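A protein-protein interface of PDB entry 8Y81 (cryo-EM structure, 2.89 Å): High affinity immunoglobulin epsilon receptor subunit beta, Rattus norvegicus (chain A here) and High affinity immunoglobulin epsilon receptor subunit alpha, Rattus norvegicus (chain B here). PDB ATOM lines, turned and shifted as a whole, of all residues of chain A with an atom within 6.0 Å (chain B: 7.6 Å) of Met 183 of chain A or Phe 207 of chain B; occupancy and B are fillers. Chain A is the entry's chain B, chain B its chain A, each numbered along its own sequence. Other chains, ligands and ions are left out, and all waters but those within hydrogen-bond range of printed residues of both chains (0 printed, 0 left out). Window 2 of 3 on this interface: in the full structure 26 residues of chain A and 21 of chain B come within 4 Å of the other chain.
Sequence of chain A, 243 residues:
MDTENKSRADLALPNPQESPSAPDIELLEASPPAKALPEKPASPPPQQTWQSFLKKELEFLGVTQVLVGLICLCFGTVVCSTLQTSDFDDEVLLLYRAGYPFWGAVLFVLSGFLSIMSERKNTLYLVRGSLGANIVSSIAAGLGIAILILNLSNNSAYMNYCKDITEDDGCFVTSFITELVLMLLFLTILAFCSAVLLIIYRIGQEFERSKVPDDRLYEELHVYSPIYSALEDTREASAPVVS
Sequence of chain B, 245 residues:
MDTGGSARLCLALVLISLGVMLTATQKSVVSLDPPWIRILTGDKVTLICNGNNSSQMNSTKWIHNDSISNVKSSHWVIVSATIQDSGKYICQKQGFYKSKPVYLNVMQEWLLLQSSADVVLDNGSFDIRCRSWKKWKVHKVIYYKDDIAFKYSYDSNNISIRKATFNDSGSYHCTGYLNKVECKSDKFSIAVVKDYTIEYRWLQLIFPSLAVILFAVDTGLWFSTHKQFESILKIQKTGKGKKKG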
ATOM      1  N   PHE A  75      18.625 -16.255  27.139  1.00  0.00           N
ATOM      2  CA  PHE A  75      17.580 -16.133  26.126  1.00  0.00           C
ATOM      3  C   PHE A  75      16.201 -16.391  26.717  1.00  0.00           C
ATOM      4  O   PHE A  75      15.239 -15.680  26.400  1.00  0.00           O
ATOM      5  CB  PHE A  75      17.856 -17.099  24.977  1.00  0.00           C
ATOM      6  CG  PHE A  75      18.918 -16.630  24.030  1.00  0.00           C
ATOM      7  CD1 PHE A  75      19.158 -15.280  23.848  1.00  0.00           C
ATOM      8  CD2 PHE A  75      19.678 -17.540  23.320  1.00  0.00           C
ATOM      9  CE1 PHE A  75      20.129 -14.854  22.971  1.00  0.00           C
ATOM     10  CE2 PHE A  75      20.653 -17.121  22.445  1.00  0.00           C
ATOM     11  CZ  PHE A  75      20.882 -15.778  22.274  1.00  0.00           C
ATOM     12  N   PHE A 176      13.009 -12.153  15.001  1.00  0.00           N
ATOM     13  CA  PHE A 176      13.925 -12.179  16.137  1.00  0.00           C
ATOM     14  C   PHE A 176      13.947 -13.552  16.791  1.00  0.00           C
ATOM     15  O   PHE A 176      15.020 -14.084  17.100  1.00  0.00           O
ATOM     16  CB  PHE A 176      13.511 -11.093  17.131  1.00  0.00           C
ATOM     17  CG  PHE A 176      13.955 -11.335  18.546  1.00  0.00           C
ATOM     18  CD1 PHE A 176      15.287 -11.227  18.909  1.00  0.00           C
ATOM     19  CD2 PHE A 176      13.023 -11.638  19.524  1.00  0.00           C
ATOM     20  CE1 PHE A 176      15.678 -11.434  20.216  1.00  0.00           C
ATOM     21  CE2 PHE A 176      13.411 -11.851  20.829  1.00  0.00           C
ATOM     22  CZ  PHE A 176      14.740 -11.746  21.174  1.00  0.00           C
ATOM     23  N   THR A 178      13.151 -16.251  15.162  1.00  0.00           N
ATOM     24  CA  THR A 178      13.702 -17.156  14.152  1.00  0.00           C
ATOM     25  C   THR A 178      15.221 -17.207  14.201  1.00  0.00           C
ATOM     26  O   THR A 178      15.810 -18.292  14.207  1.00  0.00           O
ATOM     27  CB  THR A 178      13.261 -16.739  12.753  1.00  0.00           C
ATOM     28  OG1 THR A 178      11.866 -16.425  12.758  1.00  0.00           O
ATOM     29  CG2 THR A 178      13.519 -17.863  11.765  1.00  0.00           C
ATOM     30  N   GLU A 179      15.878 -16.055  14.266  1.00  0.00           N
ATOM     31  CA  GLU A 179      17.337 -16.102  14.317  1.00  0.00           C
ATOM     32  C   GLU A 179      17.850 -16.388  15.728  1.00  0.00           C
ATOM     33  O   GLU A 179      18.968 -16.891  15.891  1.00  0.00           O
ATOM     34  CB  GLU A 179      17.931 -14.837  13.697  1.00  0.00           C
ATOM     35  CG  GLU A 179      17.382 -13.531  14.177  1.00  0.00           C
ATOM     36  CD  GLU A 179      18.117 -12.963  15.338  1.00  0.00           C
ATOM     37  OE1 GLU A 179      19.261 -13.376  15.590  1.00  0.00           O
ATOM     38  OE2 GLU A 179      17.545 -12.071  15.979  1.00  0.00           O
ATOM     39  N   LEU A 180      17.014 -16.197  16.754  1.00  0.00           N
ATOM     40  CA  LEU A 180      17.372 -16.703  18.076  1.00  0.00           C
ATOM     41  C   LEU A 180      17.236 -18.223  18.147  1.00  0.00           C
ATOM     42  O   LEU A 180      18.025 -18.878  18.824  1.00  0.00           O
ATOM     43  CB  LEU A 180      16.521 -16.006  19.141  1.00  0.00           C
ATOM     44  CG  LEU A 180      16.802 -16.169  20.637  1.00  0.00           C
ATOM     45  CD1 LEU A 180      16.449 -14.895  21.348  1.00  0.00           C
ATOM     46  CD2 LEU A 180      15.983 -17.276  21.241  1.00  0.00           C
ATOM     47  N   VAL A 181      16.256 -18.794  17.447  1.00  0.00           N
ATOM     48  CA  VAL A 181      16.162 -20.240  17.251  1.00  0.00           C
ATOM     49  C   VAL A 181      17.326 -20.754  16.416  1.00  0.00           C
ATOM     50  O   VAL A 181      17.832 -21.849  16.659  1.00  0.00           O
ATOM     51  CB  VAL A 181      14.781 -20.590  16.651  1.00  0.00           C
ATOM     52  CG1 VAL A 181      14.695 -22.003  16.173  1.00  0.00           C
ATOM     53  CG2 VAL A 181      13.746 -20.511  17.743  1.00  0.00           C
ATOM     54  N   LEU A 182      17.799 -19.963  15.453  1.00  0.00           N
ATOM     55  CA  LEU A 182      18.962 -20.366  14.664  1.00  0.00           C
ATOM     56  C   LEU A 182      20.229 -20.431  15.517  1.00  0.00           C
ATOM     57  O   LEU A 182      20.968 -21.424  15.477  1.00  0.00           O
ATOM     58  CB  LEU A 182      19.151 -19.411  13.488  1.00  0.00           C
ATOM     59  CG  LEU A 182      18.243 -19.699  12.296  1.00  0.00           C
ATOM     60  CD1 LEU A 182      18.084 -18.461  11.437  1.00  0.00           C
ATOM     61  CD2 LEU A 182      18.782 -20.863  11.487  1.00  0.00           C
ATOM     62  N   MET A 183      20.477 -19.409  16.329  1.00  0.00           N
ATOM     63  CA  MET A 183      21.651 -19.451  17.195  1.00  0.00           C
ATOM     64  C   MET A 183      21.397 -20.145  18.525  1.00  0.00           C
ATOM     65  O   MET A 183      22.293 -20.173  19.370  1.00  0.00           O
ATOM     66  CB  MET A 183      22.195 -18.050  17.445  1.00  0.00           C
ATOM     67  CG  MET A 183      21.280 -17.142  18.192  1.00  0.00           C
ATOM     68  SD  MET A 183      22.092 -15.555  18.265  1.00  0.00           S
ATOM     69  CE  MET A 183      21.901 -15.028  16.575  1.00  0.00           C
ATOM     70  N   LEU A 184      20.200 -20.674  18.746  1.00  0.00           N
ATOM     71  CA  LEU A 184      19.998 -21.687  19.770  1.00  0.00           C
ATOM     72  C   LEU A 184      20.124 -23.081  19.194  1.00  0.00           C
ATOM     73  O   LEU A 184      20.473 -24.011  19.916  1.00  0.00           O
ATOM     74  CB  LEU A 184      18.625 -21.527  20.426  1.00  0.00           C
ATOM     75  CG  LEU A 184      18.572 -20.663  21.682  1.00  0.00           C
ATOM     76  CD1 LEU A 184      17.223 -20.777  22.356  1.00  0.00           C
ATOM     77  CD2 LEU A 184      19.679 -21.065  22.628  1.00  0.00           C
ATOM     78  N   LEU A 185      19.874 -23.227  17.895  1.00  0.00           N
ATOM     79  CA  LEU A 185      20.107 -24.484  17.204  1.00  0.00           C
ATOM     80  C   LEU A 185      21.592 -24.740  17.039  1.00  0.00           C
ATOM     81  O   LEU A 185      22.041 -25.882  17.153  1.00  0.00           O
ATOM     82  CB  LEU A 185      19.405 -24.454  15.849  1.00  0.00           C
ATOM     83  CG  LEU A 185      19.330 -25.738  15.036  1.00  0.00           C
ATOM     84  CD1 LEU A 185      18.587 -26.808  15.808  1.00  0.00           C
ATOM     85  CD2 LEU A 185      18.648 -25.447  13.718  1.00  0.00           C
ATOM     86  N   PHE A 186      22.366 -23.682  16.782  1.00  0.00           N
ATOM     87  CA  PHE A 186      23.822 -23.805  16.744  1.00  0.00           C
ATOM     88  C   PHE A 186      24.375 -24.226  18.103  1.00  0.00           C
ATOM     89  O   PHE A 186      25.186 -25.160  18.199  1.00  0.00           O
ATOM     90  CB  PHE A 186      24.434 -22.480  16.287  1.00  0.00           C
ATOM     91  CG  PHE A 186      25.932 -22.434  16.369  1.00  0.00           C
ATOM     92  CD1 PHE A 186      26.711 -23.131  15.459  1.00  0.00           C
ATOM     93  CD2 PHE A 186      26.564 -21.676  17.344  1.00  0.00           C
ATOM     94  CE1 PHE A 186      28.091 -23.084  15.529  1.00  0.00           C
ATOM     95  CE2 PHE A 186      27.943 -21.626  17.419  1.00  0.00           C
ATOM     96  CZ  PHE A 186      28.706 -22.330  16.511  1.00  0.00           C
ATOM     97  N   LEU A 187      23.904 -23.583  19.174  1.00  0.00           N
ATOM     98  CA  LEU A 187      24.357 -23.933  20.515  1.00  0.00           C
ATOM     99  C   LEU A 187      23.849 -25.303  20.953  1.00  0.00           C
ATOM    100  O   LEU A 187      24.562 -26.025  21.652  1.00  0.00           O
ATOM    101  CB  LEU A 187      23.921 -22.862  21.513  1.00  0.00           C
ATOM    102  CG  LEU A 187      24.564 -21.481  21.368  1.00  0.00           C
ATOM    103  CD1 LEU A 187      23.887 -20.492  22.286  1.00  0.00           C
ATOM    104  CD2 LEU A 187      26.050 -21.531  21.647  1.00  0.00           C
ATOM    105  N   THR A 188      22.638 -25.685  20.549  1.00  0.00           N
ATOM    106  CA  THR A 188      22.110 -26.997  20.895  1.00  0.00           C
ATOM    107  C   THR A 188      22.812 -28.102  20.119  1.00  0.00           C
ATOM    108  O   THR A 188      23.021 -29.189  20.659  1.00  0.00           O
ATOM    109  CB  THR A 188      20.601 -27.021  20.648  1.00  0.00           C
ATOM    110  OG1 THR A 188      19.996 -25.919  21.329  1.00  0.00           O
ATOM    111  CG2 THR A 188      19.975 -28.303  21.169  1.00  0.00           C
ATOM    112  N   TRP B 202      14.640  -3.274  20.780  1.00  0.00           N
ATOM    113  CA  TRP B 202      15.685  -3.588  21.750  1.00  0.00           C
ATOM    114  C   TRP B 202      15.939  -5.084  21.883  1.00  0.00           C
ATOM    115  O   TRP B 202      16.963  -5.470  22.457  1.00  0.00           O
ATOM    116  CB  TRP B 202      15.339  -2.994  23.120  1.00  0.00           C
ATOM    117  CG  TRP B 202      14.223  -3.690  23.854  1.00  0.00           C
ATOM    118  CD1 TRP B 202      14.320  -4.775  24.686  1.00  0.00           C
ATOM    119  CD2 TRP B 202      12.844  -3.324  23.840  1.00  0.00           C
ATOM    120  NE1 TRP B 202      13.082  -5.111  25.168  1.00  0.00           N
ATOM    121  CE2 TRP B 202      12.159  -4.234  24.667  1.00  0.00           C
ATOM    122  CE3 TRP B 202      12.121  -2.316  23.201  1.00  0.00           C
ATOM    123  CZ2 TRP B 202      10.787  -4.164  24.872  1.00  0.00           C
ATOM    124  CZ3 TRP B 202      10.765  -2.246  23.410  1.00  0.00           C
ATOM    125  CH2 TRP B 202      10.108  -3.165  24.234  1.00  0.00           C
ATOM    126  N   LEU B 203      15.024  -5.924  21.392  1.00  0.00           N
ATOM    127  CA  LEU B 203      15.284  -7.355  21.305  1.00  0.00           C
ATOM    128  C   LEU B 203      16.462  -7.639  20.385  1.00  0.00           C
ATOM    129  O   LEU B 203      17.294  -8.504  20.679  1.00  0.00           O
ATOM    130  CB  LEU B 203      14.034  -8.078  20.820  1.00  0.00           C
ATOM    131  CG  LEU B 203      12.863  -8.066  21.798  1.00  0.00           C
ATOM    132  CD1 LEU B 203      11.647  -8.660  21.133  1.00  0.00           C
ATOM    133  CD2 LEU B 203      13.213  -8.828  23.059  1.00  0.00           C
ATOM    134  N   GLN B 204      16.592  -6.879  19.295  1.00  0.00           N
ATOM    135  CA  GLN B 204      17.798  -7.020  18.488  1.00  0.00           C
ATOM    136  C   GLN B 204      19.024  -6.421  19.154  1.00  0.00           C
ATOM    137  O   GLN B 204      20.130  -6.608  18.642  1.00  0.00           O
ATOM    138  CB  GLN B 204      17.620  -6.390  17.114  1.00  0.00           C
ATOM    139  CG  GLN B 204      16.639  -7.117  16.238  1.00  0.00           C
ATOM    140  CD  GLN B 204      17.044  -8.544  15.974  1.00  0.00           C
ATOM    141  OE1 GLN B 204      16.411  -9.471  16.466  1.00  0.00           O
ATOM    142  NE2 GLN B 204      18.107  -8.731  15.207  1.00  0.00           N
ATOM    143  N   LEU B 205      18.855  -5.693  20.253  1.00  0.00           N
ATOM    144  CA  LEU B 205      19.955  -5.270  21.102  1.00  0.00           C
ATOM    145  C   LEU B 205      20.307  -6.306  22.159  1.00  0.00           C
ATOM    146  O   LEU B 205      21.182  -6.037  22.986  1.00  0.00           O
ATOM    147  CB  LEU B 205      19.628  -3.937  21.784  1.00  0.00           C
ATOM    148  CG  LEU B 205      19.939  -2.621  21.059  1.00  0.00           C
ATOM    149  CD1 LEU B 205      19.015  -2.363  19.879  1.00  0.00           C
ATOM    150  CD2 LEU B 205      19.871  -1.469  22.042  1.00  0.00           C
ATOM    151  N   ILE B 206      19.636  -7.462  22.175  1.00  0.00           N
ATOM    152  CA  ILE B 206      20.030  -8.521  23.101  1.00  0.00           C
ATOM    153  C   ILE B 206      21.355  -9.145  22.675  1.00  0.00           C
ATOM    154  O   ILE B 206      22.247  -9.370  23.500  1.00  0.00           O
ATOM    155  CB  ILE B 206      18.906  -9.568  23.227  1.00  0.00           C
ATOM    156  CG1 ILE B 206      17.660  -8.937  23.852  1.00  0.00           C
ATOM    157  CG2 ILE B 206      19.353 -10.769  24.043  1.00  0.00           C
ATOM    158  CD1 ILE B 206      17.879  -8.395  25.243  1.00  0.00           C
ATOM    159  N   PHE B 207      21.518  -9.405  21.384  1.00  0.00           N
ATOM    160  CA  PHE B 207      22.705 -10.065  20.841  1.00  0.00           C
ATOM    161  C   PHE B 207      24.003  -9.250  20.866  1.00  0.00           C
ATOM    162  O   PHE B 207      25.051  -9.845  21.146  1.00  0.00           O
ATOM    163  CB  PHE B 207      22.409 -10.550  19.422  1.00  0.00           C
ATOM    164  CG  PHE B 207      21.134 -11.303  19.323  1.00  0.00           C
ATOM    165  CD1 PHE B 207      21.038 -12.585  19.828  1.00  0.00           C
ATOM    166  CD2 PHE B 207      20.017 -10.716  18.767  1.00  0.00           C
ATOM    167  CE1 PHE B 207      19.851 -13.280  19.756  1.00  0.00           C
ATOM    168  CE2 PHE B 207      18.835 -11.400  18.701  1.00  0.00           C
ATOM    169  CZ  PHE B 207      18.751 -12.689  19.186  1.00  0.00           C
ATOM    170  N   PRO B 208      24.034  -7.938  20.564  1.00  0.00           N
ATOM    171  CA  PRO B 208      25.275  -7.202  20.848  1.00  0.00           C
ATOM    172  C   PRO B 208      25.542  -7.067  22.330  1.00  0.00           C
ATOM    173  O   PRO B 208      26.714  -7.057  22.729  1.00  0.00           O
ATOM    174  CB  PRO B 208      25.041  -5.838  20.186  1.00  0.00           C
ATOM    175  CG  PRO B 208      23.598  -5.687  20.161  1.00  0.00           C
ATOM    176  CD  PRO B 208      23.081  -7.051  19.871  1.00  0.00           C
ATOM    177  N   SER B 209      24.488  -6.974  23.152  1.00  0.00           N
ATOM    178  CA  SER B 209      24.658  -7.031  24.598  1.00  0.00           C
ATOM    179  C   SER B 209      25.261  -8.359  25.017  1.00  0.00           C
ATOM    180  O   SER B 209      26.239  -8.390  25.765  1.00  0.00           O
ATOM    181  CB  SER B 209      23.325  -6.802  25.304  1.00  0.00           C
ATOM    182  OG  SER B 209      23.420  -7.123  26.679  1.00  0.00           O
ATOM    183  N   LEU B 210      24.778  -9.463  24.456  1.00  0.00           N
ATOM    184  CA  LEU B 210      25.426 -10.742  24.718  1.00  0.00           C
ATOM    185  C   LEU B 210      26.730 -10.933  23.955  1.00  0.00           C
ATOM    186  O   LEU B 210      27.303 -12.025  24.016  1.00  0.00           O
ATOM    187  CB  LEU B 210      24.469 -11.895  24.429  1.00  0.00           C
ATOM    188  CG  LEU B 210      23.322 -11.908  25.433  1.00  0.00           C
ATOM    189  CD1 LEU B 210      22.301 -12.954  25.081  1.00  0.00           C
ATOM    190  CD2 LEU B 210      23.887 -12.157  26.819  1.00  0.00           C
ATOM    191  N   ALA B 211      27.208  -9.919  23.234  1.00  0.00           N
ATOM    192  CA  ALA B 211      28.624  -9.869  22.913  1.00  0.00           C
ATOM    193  C   ALA B 211      29.411  -9.198  24.033  1.00  0.00           C
ATOM    194  O   ALA B 211      30.470  -9.694  24.430  1.00  0.00           O
ATOM    195  CB  ALA B 211      28.839  -9.141  21.588  1.00  0.00           C
ATOM    196  N   VAL B 212      28.887  -8.099  24.595  1.00  0.00           N
ATOM    197  CA  VAL B 212      29.664  -7.306  25.548  1.00  0.00           C
ATOM    198  C   VAL B 212      29.727  -7.924  26.936  1.00  0.00           C
ATOM    199  O   VAL B 212      30.446  -7.397  27.793  1.00  0.00           O
ATOM    200  CB  VAL B 212      29.163  -5.850  25.676  1.00  0.00           C
ATOM    201  CG1 VAL B 212      28.985  -5.220  24.309  1.00  0.00           C
ATOM    202  CG2 VAL B 212      27.896  -5.740  26.511  1.00  0.00           C
ATOM    203  N   ILE B 213      28.998  -9.010  27.201  1.00  0.00           N
ATOM    204  CA  ILE B 213      29.424  -9.914  28.269  1.00  0.00           C
ATOM    205  C   ILE B 213      30.521 -10.846  27.775  1.00  0.00           C
ATOM    206  O   ILE B 213      31.613 -10.883  28.357  1.00  0.00           O
ATOM    207  CB  ILE B 213      28.251 -10.712  28.884  1.00  0.00           C
ATOM    208  CG1 ILE B 213      27.209  -9.833  29.597  1.00  0.00           C
ATOM    209  CG2 ILE B 213      28.769 -11.783  29.834  1.00  0.00           C
ATOM    210  CD1 ILE B 213      26.082  -9.311  28.799  1.00  0.00           C
ATOM    211  N   LEU B 214      30.256 -11.565  26.673  1.00  0.00           N
ATOM    212  CA  LEU B 214      31.113 -12.674  26.244  1.00  0.00           C
ATOM    213  C   LEU B 214      32.515 -12.202  25.882  1.00  0.00           C
ATOM    214  O   LEU B 214      33.508 -12.780  26.341  1.00  0.00           O
ATOM    215  CB  LEU B 214      30.486 -13.400  25.056  1.00  0.00           C
ATOM    216  CG  LEU B 214      29.401 -14.431  25.348  1.00  0.00           C
ATOM    217  CD1 LEU B 214      28.846 -14.956  24.049  1.00  0.00           C
ATOM    218  CD2 LEU B 214      29.945 -15.563  26.194  1.00  0.00           C
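The side-chain carboxylate of Glu 179 of chain A sits close to the side-chain amide oxygen of Gln 204 of chain B.
Among the printed residues, pairs that only touch across the chains: Glu 179 of chain A with Phe 207 of chain B, Phe 176 of chain A with Gln 204 of chain B, Phe 176 of chain A with Leu 203 of chain B, Phe 176 of chain A with Phe 207 of chain B, Met 183 of chain A with Phe 207 of chain B, Phe 75 of chain A with Leu 210 of chain B, Phe 75 of chain A with Phe 207 of chain B and Leu 180 of chain A with Phe 207 of chain B.
Printed residues of chain B within 4 Å of Met 183 of chain A: Phe 207. Of the printed residues of chain A, Phe 207 of chain B touches Phe 75, Phe 176, Glu 179, Leu 180 and Met 183. Printed residues of chain A within 4 Å of Gln 204 of chain B: Phe 176 and Glu 179. Of the printed residues of chain B, Glu 179 of chain A touches Gln 204 (2.9 Å) and Phe 207 (3.1 Å). Of the printed residues of chain B, Phe 75 of chain A touches Phe 207 (3.6 Å) and Leu 210 (3.6 Å). Printed residues of chain B within 4 Å of Leu 180 of chain A: Phe 207. The nearest residue of chain B that does not touch Met 183 of chain A is Leu 210 of chain B (7.3 Å). The nearest printed residue of chain B that does not touch Glu 179 of chain A is Leu 203 of chain B (5.9 Å).
Hydrophobic or aromatic side chains of chain A within 4 Å of the printed part of chain B: Phe 75, Phe 176, Leu 180 and Met 183. Of the 13 printed residues of chain B, 4 touch a printed residue of chain A. Printed residues of chain B that touch a printed residue of chain A: Leu 203, Gln 204, Phe 207 and Leu 210. Among the printed residues, 9 pairs touch across the chains.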
